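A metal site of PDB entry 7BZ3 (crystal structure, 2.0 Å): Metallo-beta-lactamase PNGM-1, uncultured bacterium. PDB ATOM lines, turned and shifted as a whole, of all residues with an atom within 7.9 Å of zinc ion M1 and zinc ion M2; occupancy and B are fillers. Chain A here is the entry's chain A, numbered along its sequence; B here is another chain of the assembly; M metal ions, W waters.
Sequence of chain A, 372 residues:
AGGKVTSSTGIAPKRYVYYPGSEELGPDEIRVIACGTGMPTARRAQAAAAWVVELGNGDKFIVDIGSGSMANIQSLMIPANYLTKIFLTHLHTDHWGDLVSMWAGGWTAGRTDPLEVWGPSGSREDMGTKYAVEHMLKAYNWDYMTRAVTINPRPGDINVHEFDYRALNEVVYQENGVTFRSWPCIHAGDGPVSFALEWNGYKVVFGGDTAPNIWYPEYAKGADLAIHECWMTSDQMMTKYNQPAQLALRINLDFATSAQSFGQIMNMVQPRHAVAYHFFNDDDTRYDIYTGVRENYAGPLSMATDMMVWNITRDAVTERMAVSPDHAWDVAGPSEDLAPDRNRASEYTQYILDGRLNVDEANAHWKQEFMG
The side-chain carboxylate (OD2) of Asp 64 sits at hydrogen-bond distance from a ring nitrogen (ND1) of His 95 (2.6 Å). OG1 of Thr 89 lies within hydrogen-bond range of ND1 of His 90 (3.0 Å). The backbone carbonyl oxygen (O) of Asp 94 sits at hydrogen-bond distance from the backbone NH (N) of Ala 49 (2.9 Å). The side-chain carboxylate (OD1) of Asp 209 lies within hydrogen-bond range of the side-chain hydroxyl (OH) of Tyr 277 (3.2 Å). ND1 of His 278 sits at hydrogen-bond distance from O of Gly 38 (3.4 Å). The side-chain sulfur (SD) of Met 39 lies within hydrogen-bond range of a ring nitrogen (ND1) of His 278 (3.6 Å).
Within 4 Å of zinc ion M1: Asp 94, His 95, Asp 209 and His 278. The nearest printed residue that does not touch zinc ion M1 is His 90 (4.2 Å).
Of the 26 residues printed, 5 come within 4 Å of zinc ion M2.
Zinc ion M1 is bound by water W1 (1.9 Å), NE2 of His 278 (2.0 Å), NE2 of His 95 (2.1 Å), OD2 of Asp 209 (2.1 Å) and OD2 of Asp 94 (2.2 Å). Zinc ion M1 has five donor atoms within binding distance.
Zinc ion M2 is bound by water W1 (1.9 Å), a ring nitrogen (NE2) of His 187 (2.1 Å), a ring nitrogen (ND1) of His 92 (2.1 Å), a ring nitrogen (NE2) of His 90 (2.2 Å) and the side-chain carboxylate (OD2) of Asp 209 (2.5 Å).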
ATOM      1  N   GLY A  38      19.569  14.245 -15.102  1.00  0.00           N
ATOM      2  CA  GLY A  38      20.261  14.172 -13.794  1.00  0.00           C
ATOM      3  C   GLY A  38      21.760  14.205 -13.944  1.00  0.00           C
ATOM      4  O   GLY A  38      22.231  14.934 -14.806  1.00  0.00           O
ATOM      5  N   MET A  39      22.476  13.391 -13.176  1.00  0.00           N
ATOM      6  CA  MET A  39      23.940  13.519 -12.963  1.00  0.00           C
ATOM      7  C   MET A  39      24.641  12.165 -13.133  1.00  0.00           C
ATOM      8  O   MET A  39      23.996  11.159 -13.372  1.00  0.00           O
ATOM      9  CB  MET A  39      24.182  14.046 -11.534  1.00  0.00           C
ATOM     10  CG  MET A  39      23.501  15.389 -11.242  1.00  0.00           C
ATOM     11  SD  MET A  39      24.552  16.728 -11.800  1.00  0.00           S
ATOM     12  CE  MET A  39      25.830  16.741 -10.533  1.00  0.00           C
ATOM     13  N   PRO A  40      25.982  12.087 -12.981  1.00  0.00           N
ATOM     14  CA  PRO A  40      26.641  10.779 -12.934  1.00  0.00           C
ATOM     15  C   PRO A  40      26.256  10.005 -11.654  1.00  0.00           C
ATOM     16  O   PRO A  40      26.456   8.798 -11.644  1.00  0.00           O
ATOM     17  CB  PRO A  40      28.143  11.068 -13.011  1.00  0.00           C
ATOM     18  CG  PRO A  40      28.270  12.567 -13.288  1.00  0.00           C
ATOM     19  CD  PRO A  40      26.936  13.207 -12.916  1.00  0.00           C
ATOM     20  N   ALA A  48      20.234   9.688 -15.889  1.00  0.00           N
ATOM     21  CA  ALA A  48      21.293  10.448 -16.618  1.00  0.00           C
ATOM     22  C   ALA A  48      20.775  10.893 -18.004  1.00  0.00           C
ATOM     23  O   ALA A  48      19.823  10.262 -18.523  1.00  0.00           O
ATOM     24  CB  ALA A  48      22.533   9.620 -16.751  1.00  0.00           C
ATOM     25  N   ALA A  49      21.466  11.837 -18.651  1.00  0.00           N
ATOM     26  CA  ALA A  49      20.987  12.661 -19.790  1.00  0.00           C
ATOM     27  C   ALA A  49      20.479  11.802 -20.958  1.00  0.00           C
ATOM     28  O   ALA A  49      21.231  10.980 -21.482  1.00  0.00           O
ATOM     29  CB  ALA A  49      22.085  13.603 -20.229  1.00  0.00           C
ATOM     30  N   ASP A  64      21.746  11.649 -26.652  1.00  0.00           N
ATOM     31  CA  ASP A  64      22.308  11.153 -25.371  1.00  0.00           C
ATOM     32  C   ASP A  64      21.460   9.989 -24.846  1.00  0.00           C
ATOM     33  O   ASP A  64      20.244   9.893 -25.172  1.00  0.00           O
ATOM     34  CB  ASP A  64      22.546  12.287 -24.374  1.00  0.00           C
ATOM     35  CG  ASP A  64      23.762  13.156 -24.713  1.00  0.00           C
ATOM     36  OD1 ASP A  64      24.498  12.797 -25.691  1.00  0.00           O
ATOM     37  OD2 ASP A  64      23.972  14.209 -24.013  1.00  0.00           O
ATOM     38  N   THR A  89      26.665  13.635 -27.442  1.00  0.00           N
ATOM     39  CA  THR A  89      27.352  14.960 -27.292  1.00  0.00           C
ATOM     40  C   THR A  89      28.797  14.694 -26.902  1.00  0.00           C
ATOM     41  O   THR A  89      29.667  15.477 -27.340  1.00  0.00           O
ATOM     42  CB  THR A  89      26.613  15.856 -26.291  1.00  0.00           C
ATOM     43  OG1 THR A  89      26.503  15.226 -25.009  1.00  0.00           O
ATOM     44  CG2 THR A  89      25.220  16.207 -26.754  1.00  0.00           C
ATOM     45  N   HIS A  90      29.011  13.619 -26.118  1.00  0.00           N
ATOM     46  CA  HIS A  90      30.317  13.251 -25.517  1.00  0.00           C
ATOM     47  C   HIS A  90      30.257  11.890 -24.815  1.00  0.00           C
ATOM     48  O   HIS A  90      29.171  11.251 -24.727  1.00  0.00           O
ATOM     49  CB  HIS A  90      30.861  14.396 -24.659  1.00  0.00           C
ATOM     50  CG  HIS A  90      30.192  14.605 -23.347  1.00  0.00           C
ATOM     51  ND1 HIS A  90      28.879  14.993 -23.238  1.00  0.00           N
ATOM     52  CD2 HIS A  90      30.696  14.556 -22.098  1.00  0.00           C
ATOM     53  CE1 HIS A  90      28.597  15.120 -21.964  1.00  0.00           C
ATOM     54  NE2 HIS A  90      29.687  14.857 -21.248  1.00  0.00           N
ATOM     55  N   LEU A  91      31.425  11.453 -24.355  1.00  0.00           N
ATOM     56  CA  LEU A  91      31.658  10.039 -23.909  1.00  0.00           C
ATOM     57  C   LEU A  91      31.714   9.883 -22.391  1.00  0.00           C
ATOM     58  O   LEU A  91      32.241   8.839 -21.937  1.00  0.00           O
ATOM     59  CB  LEU A  91      32.919   9.560 -24.626  1.00  0.00           C
ATOM     60  CG  LEU A  91      32.760   9.518 -26.134  1.00  0.00           C
ATOM     61  CD1 LEU A  91      34.096   9.366 -26.780  1.00  0.00           C
ATOM     62  CD2 LEU A  91      31.779   8.439 -26.564  1.00  0.00           C
ATOM     63  N   HIS A  92      31.085  10.754 -21.604  1.00  0.00           N
ATOM     64  CA  HIS A  92      30.813  10.478 -20.152  1.00  0.00           C
ATOM     65  C   HIS A  92      29.743   9.395 -20.013  1.00  0.00           C
ATOM     66  O   HIS A  92      28.816   9.392 -20.805  1.00  0.00           O
ATOM     67  CB  HIS A  92      30.434  11.711 -19.369  1.00  0.00           C
ATOM     68  CG  HIS A  92      31.601  12.494 -18.861  1.00  0.00           C
ATOM     69  ND1 HIS A  92      31.598  13.860 -18.873  1.00  0.00           N
ATOM     70  CD2 HIS A  92      32.785  12.117 -18.364  1.00  0.00           C
ATOM     71  CE1 HIS A  92      32.720  14.301 -18.344  1.00  0.00           C
ATOM     72  NE2 HIS A  92      33.474  13.251 -18.031  1.00  0.00           N
ATOM     73  N   THR A  93      29.837   8.561 -18.980  1.00  0.00           N
ATOM     74  CA  THR A  93      28.826   7.499 -18.690  1.00  0.00           C
ATOM     75  C   THR A  93      27.398   8.109 -18.651  1.00  0.00           C
ATOM     76  O   THR A  93      26.494   7.462 -19.166  1.00  0.00           O
ATOM     77  CB  THR A  93      29.106   6.779 -17.365  1.00  0.00           C
ATOM     78  OG1 THR A  93      29.164   7.752 -16.315  1.00  0.00           O
ATOM     79  CG2 THR A  93      30.370   5.949 -17.386  1.00  0.00           C
ATOM     80  N   ASP A  94      27.206   9.323 -18.099  1.00  0.00           N
ATOM     81  CA  ASP A  94      25.863   9.936 -17.896  1.00  0.00           C
ATOM     82  C   ASP A  94      25.272  10.427 -19.238  1.00  0.00           C
ATOM     83  O   ASP A  94      24.154  10.962 -19.161  1.00  0.00           O
ATOM     84  CB  ASP A  94      25.829  11.054 -16.829  1.00  0.00           C
ATOM     85  CG  ASP A  94      26.759  12.240 -17.051  1.00  0.00           C
ATOM     86  OD1 ASP A  94      27.955  12.030 -17.257  1.00  0.00           O
ATOM     87  OD2 ASP A  94      26.264  13.384 -17.029  1.00  0.00           O
ATOM     88  N   HIS A  95      25.950  10.182 -20.377  1.00  0.00           N
ATOM     89  CA  HIS A  95      25.483  10.528 -21.744  1.00  0.00           C
ATOM     90  C   HIS A  95      25.406   9.345 -22.710  1.00  0.00           C
ATOM     91  O   HIS A  95      24.734   9.513 -23.703  1.00  0.00           O
ATOM     92  CB  HIS A  95      26.360  11.636 -22.354  1.00  0.00           C
ATOM     93  CG  HIS A  95      26.253  12.868 -21.549  1.00  0.00           C
ATOM     94  ND1 HIS A  95      25.332  13.855 -21.865  1.00  0.00           N
ATOM     95  CD2 HIS A  95      26.786  13.175 -20.344  1.00  0.00           C
ATOM     96  CE1 HIS A  95      25.409  14.794 -20.953  1.00  0.00           C
ATOM     97  NE2 HIS A  95      26.296  14.400 -19.986  1.00  0.00           N
ATOM     98  N   HIS A 187      34.625  20.987 -21.817  1.00  0.00           N
ATOM     99  CA  HIS A 187      34.148  19.994 -20.827  1.00  0.00           C
ATOM    100  C   HIS A 187      35.159  18.853 -20.697  1.00  0.00           C
ATOM    101  O   HIS A 187      35.223  17.965 -21.607  1.00  0.00           O
ATOM    102  CB  HIS A 187      32.728  19.602 -21.211  1.00  0.00           C
ATOM    103  CG  HIS A 187      32.118  18.605 -20.306  1.00  0.00           C
ATOM    104  ND1 HIS A 187      31.806  18.880 -18.984  1.00  0.00           N
ATOM    105  CD2 HIS A 187      31.790  17.311 -20.503  1.00  0.00           C
ATOM    106  CE1 HIS A 187      31.269  17.809 -18.432  1.00  0.00           C
ATOM    107  NE2 HIS A 187      31.268  16.846 -19.350  1.00  0.00           N
ATOM    108  N   ALA A 188      35.917  18.885 -19.584  1.00  0.00           N
ATOM    109  CA  ALA A 188      36.836  17.824 -19.102  1.00  0.00           C
ATOM    110  C   ALA A 188      38.035  17.709 -20.047  1.00  0.00           C
ATOM    111  O   ALA A 188      39.175  17.597 -19.550  1.00  0.00           O
ATOM    112  CB  ALA A 188      36.076  16.528 -18.956  1.00  0.00           C
ATOM    113  N   PRO A 192      33.842  16.854 -26.666  1.00  0.00           N
ATOM    114  CA  PRO A 192      32.427  17.162 -26.496  1.00  0.00           C
ATOM    115  C   PRO A 192      31.887  18.282 -27.377  1.00  0.00           C
ATOM    116  O   PRO A 192      32.606  19.245 -27.692  1.00  0.00           O
ATOM    117  CB  PRO A 192      32.314  17.603 -25.025  1.00  0.00           C
ATOM    118  CG  PRO A 192      33.459  16.870 -24.346  1.00  0.00           C
ATOM    119  CD  PRO A 192      34.564  16.938 -25.377  1.00  0.00           C
ATOM    120  N   GLY A 208      24.348  19.541 -24.569  1.00  0.00           N
ATOM    121  CA  GLY A 208      25.295  18.606 -23.924  1.00  0.00           C
ATOM    122  C   GLY A 208      25.868  19.188 -22.645  1.00  0.00           C
ATOM    123  O   GLY A 208      25.141  19.867 -21.899  1.00  0.00           O
ATOM    124  N   ASP A 209      27.150  18.975 -22.396  1.00  0.00           N
ATOM    125  CA  ASP A 209      27.816  19.564 -21.225  1.00  0.00           C
ATOM    126  C   ASP A 209      28.870  20.562 -21.679  1.00  0.00           C
ATOM    127  O   ASP A 209      29.669  20.189 -22.543  1.00  0.00           O
ATOM    128  CB  ASP A 209      28.508  18.521 -20.372  1.00  0.00           C
ATOM    129  CG  ASP A 209      27.553  17.546 -19.714  1.00  0.00           C
ATOM    130  OD1 ASP A 209      26.336  17.543 -20.066  1.00  0.00           O
ATOM    131  OD2 ASP A 209      28.048  16.773 -18.899  1.00  0.00           O
ATOM    132  N   THR A 210      28.915  21.717 -21.023  1.00  0.00           N
ATOM    133  CA  THR A 210      29.961  22.727 -21.298  1.00  0.00           C
ATOM    134  C   THR A 210      30.059  23.714 -20.137  1.00  0.00           C
ATOM    135  O   THR A 210      29.050  23.912 -19.461  1.00  0.00           O
ATOM    136  CB  THR A 210      29.660  23.443 -22.623  1.00  0.00           C
ATOM    137  OG1 THR A 210      30.788  24.235 -22.951  1.00  0.00           O
ATOM    138  CG2 THR A 210      28.427  24.318 -22.554  1.00  0.00           C
ATOM    139  N   GLU A 229      23.219  22.924 -20.071  1.00  0.00           N
ATOM    140  CA  GLU A 229      23.575  22.530 -18.695  1.00  0.00           C
ATOM    141  C   GLU A 229      23.365  23.759 -17.774  1.00  0.00           C
ATOM    142  O   GLU A 229      23.710  24.920 -18.169  1.00  0.00           O
ATOM    143  CB  GLU A 229      24.975  21.929 -18.726  1.00  0.00           C
ATOM    144  CG  GLU A 229      25.706  21.917 -17.410  1.00  0.00           C
ATOM    145  CD  GLU A 229      27.220  21.924 -17.587  1.00  0.00           C
ATOM    146  OE1 GLU A 229      27.753  21.223 -18.511  1.00  0.00           O
ATOM    147  OE2 GLU A 229      27.870  22.655 -16.787  1.00  0.00           O
ATOM    148  N   TRP A 231      23.911  24.324 -13.495  1.00  0.00           N
ATOM    149  CA  TRP A 231      24.509  23.578 -12.356  1.00  0.00           C
ATOM    150  C   TRP A 231      23.809  23.922 -11.045  1.00  0.00           C
ATOM    151  O   TRP A 231      23.295  25.026 -10.910  1.00  0.00           O
ATOM    152  CB  TRP A 231      26.017  23.790 -12.257  1.00  0.00           C
ATOM    153  CG  TRP A 231      26.725  22.553 -11.802  1.00  0.00           C
ATOM    154  CD1 TRP A 231      27.171  22.249 -10.549  1.00  0.00           C
ATOM    155  CD2 TRP A 231      26.993  21.395 -12.615  1.00  0.00           C
ATOM    156  NE1 TRP A 231      27.723  20.994 -10.541  1.00  0.00           N
ATOM    157  CE2 TRP A 231      27.642  20.448 -11.792  1.00  0.00           C
ATOM    158  CE3 TRP A 231      26.753  21.062 -13.947  1.00  0.00           C
ATOM    159  CZ2 TRP A 231      28.063  19.208 -12.272  1.00  0.00           C
ATOM    160  CZ3 TRP A 231      27.169  19.845 -14.419  1.00  0.00           C
ATOM    161  CH2 TRP A 231      27.818  18.930 -13.587  1.00  0.00           C
ATOM    162  N   TYR A 277      18.942  21.975 -17.528  1.00  0.00           N
ATOM    163  CA  TYR A 277      19.028  20.540 -17.166  1.00  0.00           C
ATOM    164  C   TYR A 277      20.394  20.270 -16.529  1.00  0.00           C
ATOM    165  O   TYR A 277      21.241  21.196 -16.405  1.00  0.00           O
ATOM    166  CB  TYR A 277      18.677  19.670 -18.396  1.00  0.00           C
ATOM    167  CG  TYR A 277      19.867  19.129 -19.132  1.00  0.00           C
ATOM    168  CD1 TYR A 277      20.741  19.984 -19.775  1.00  0.00           C
ATOM    169  CD2 TYR A 277      20.181  17.781 -19.128  1.00  0.00           C
ATOM    170  CE1 TYR A 277      21.865  19.520 -20.429  1.00  0.00           C
ATOM    171  CE2 TYR A 277      21.297  17.286 -19.810  1.00  0.00           C
ATOM    172  CZ  TYR A 277      22.149  18.169 -20.456  1.00  0.00           C
ATOM    173  OH  TYR A 277      23.276  17.747 -21.112  1.00  0.00           O
ATOM    174  N   HIS A 278      20.549  19.051 -16.028  1.00  0.00           N
ATOM    175  CA  HIS A 278      21.812  18.460 -15.524  1.00  0.00           C
ATOM    176  C   HIS A 278      22.039  18.909 -14.070  1.00  0.00           C
ATOM    177  O   HIS A 278      23.205  19.130 -13.675  1.00  0.00           O
ATOM    178  CB  HIS A 278      22.970  18.821 -16.453  1.00  0.00           C
ATOM    179  CG  HIS A 278      24.049  17.796 -16.498  1.00  0.00           C
ATOM    180  ND1 HIS A 278      24.604  17.254 -15.335  1.00  0.00           N
ATOM    181  CD2 HIS A 278      24.648  17.183 -17.545  1.00  0.00           C
ATOM    182  CE1 HIS A 278      25.519  16.348 -15.696  1.00  0.00           C
ATOM    183  NE2 HIS A 278      25.573  16.309 -17.066  1.00  0.00           N
ATOM    184  N   TRP B 142      38.032   7.895 -22.913  1.00  0.00           N
ATOM    185  CA  TRP B 142      37.905   9.373 -22.918  1.00  0.00           C
ATOM    186  C   TRP B 142      37.632   9.831 -21.476  1.00  0.00           C
ATOM    187  O   TRP B 142      38.423  10.691 -20.960  1.00  0.00           O
ATOM    188  CB  TRP B 142      36.858   9.847 -23.928  1.00  0.00           C
ATOM    189  CG  TRP B 142      36.779  11.340 -23.962  1.00  0.00           C
ATOM    190  CD1 TRP B 142      37.526  12.165 -24.739  1.00  0.00           C
ATOM    191  CD2 TRP B 142      35.945  12.193 -23.152  1.00  0.00           C
ATOM    192  NE1 TRP B 142      37.215  13.474 -24.479  1.00  0.00           N
ATOM    193  CE2 TRP B 142      36.257  13.524 -23.510  1.00  0.00           C
ATOM    194  CE3 TRP B 142      34.984  11.973 -22.154  1.00  0.00           C
ATOM    195  CZ2 TRP B 142      35.656  14.618 -22.897  1.00  0.00           C
ATOM    196  CZ3 TRP B 142      34.384  13.066 -21.551  1.00  0.00           C
ATOM    197  CH2 TRP B 142      34.729  14.366 -21.916  1.00  0.00           C
ATOM    198  N   ASP B 143      36.619   9.241 -20.827  1.00  0.00           N
ATOM    199  CA  ASP B 143      36.199   9.461 -19.405  1.00  0.00           C
ATOM    200  C   ASP B 143      37.408   9.321 -18.462  1.00  0.00           C
ATOM    201  O   ASP B 143      37.691  10.281 -17.702  1.00  0.00           O
ATOM    202  CB  ASP B 143      35.108   8.475 -18.963  1.00  0.00           C
ATOM    203  CG  ASP B 143      34.421   8.827 -17.641  1.00  0.00           C
ATOM    204  OD1 ASP B 143      34.929   9.692 -16.926  1.00  0.00           O
ATOM    205  OD2 ASP B 143      33.338   8.300 -17.380  1.00  0.00           O
ATOM    206  N   ARG B 147      39.391  12.632 -16.747  1.00  0.00           N
ATOM    207  CA  ARG B 147      39.203  12.698 -15.264  1.00  0.00           C
ATOM    208  C   ARG B 147      40.549  12.586 -14.538  1.00  0.00           C
ATOM    209  O   ARG B 147      40.697  13.298 -13.527  1.00  0.00           O
ATOM    210  CB  ARG B 147      38.321  11.556 -14.743  1.00  0.00           C
ATOM    211  CG  ARG B 147      37.967  11.664 -13.260  1.00  0.00           C
ATOM    212  CD  ARG B 147      36.744  10.839 -12.925  1.00  0.00           C
ATOM    213  NE  ARG B 147      35.575  11.314 -13.678  1.00  0.00           N
ATOM    214  CZ  ARG B 147      34.484  10.582 -13.965  1.00  0.00           C
ATOM    215  NH1 ARG B 147      34.403   9.327 -13.563  1.00  0.00           N
ATOM    216  NH2 ARG B 147      33.489  11.120 -14.666  1.00  0.00           N
HETATM  217 ZN    ZN M   1      26.837  15.201 -18.131  1.00  0.00          ZN
HETATM  218 ZN    ZN M   2      29.965  15.231 -19.145  1.00  0.00          ZN
HETATM  219  O   HOH W   1      28.678  14.700 -17.839  1.00  0.00           O
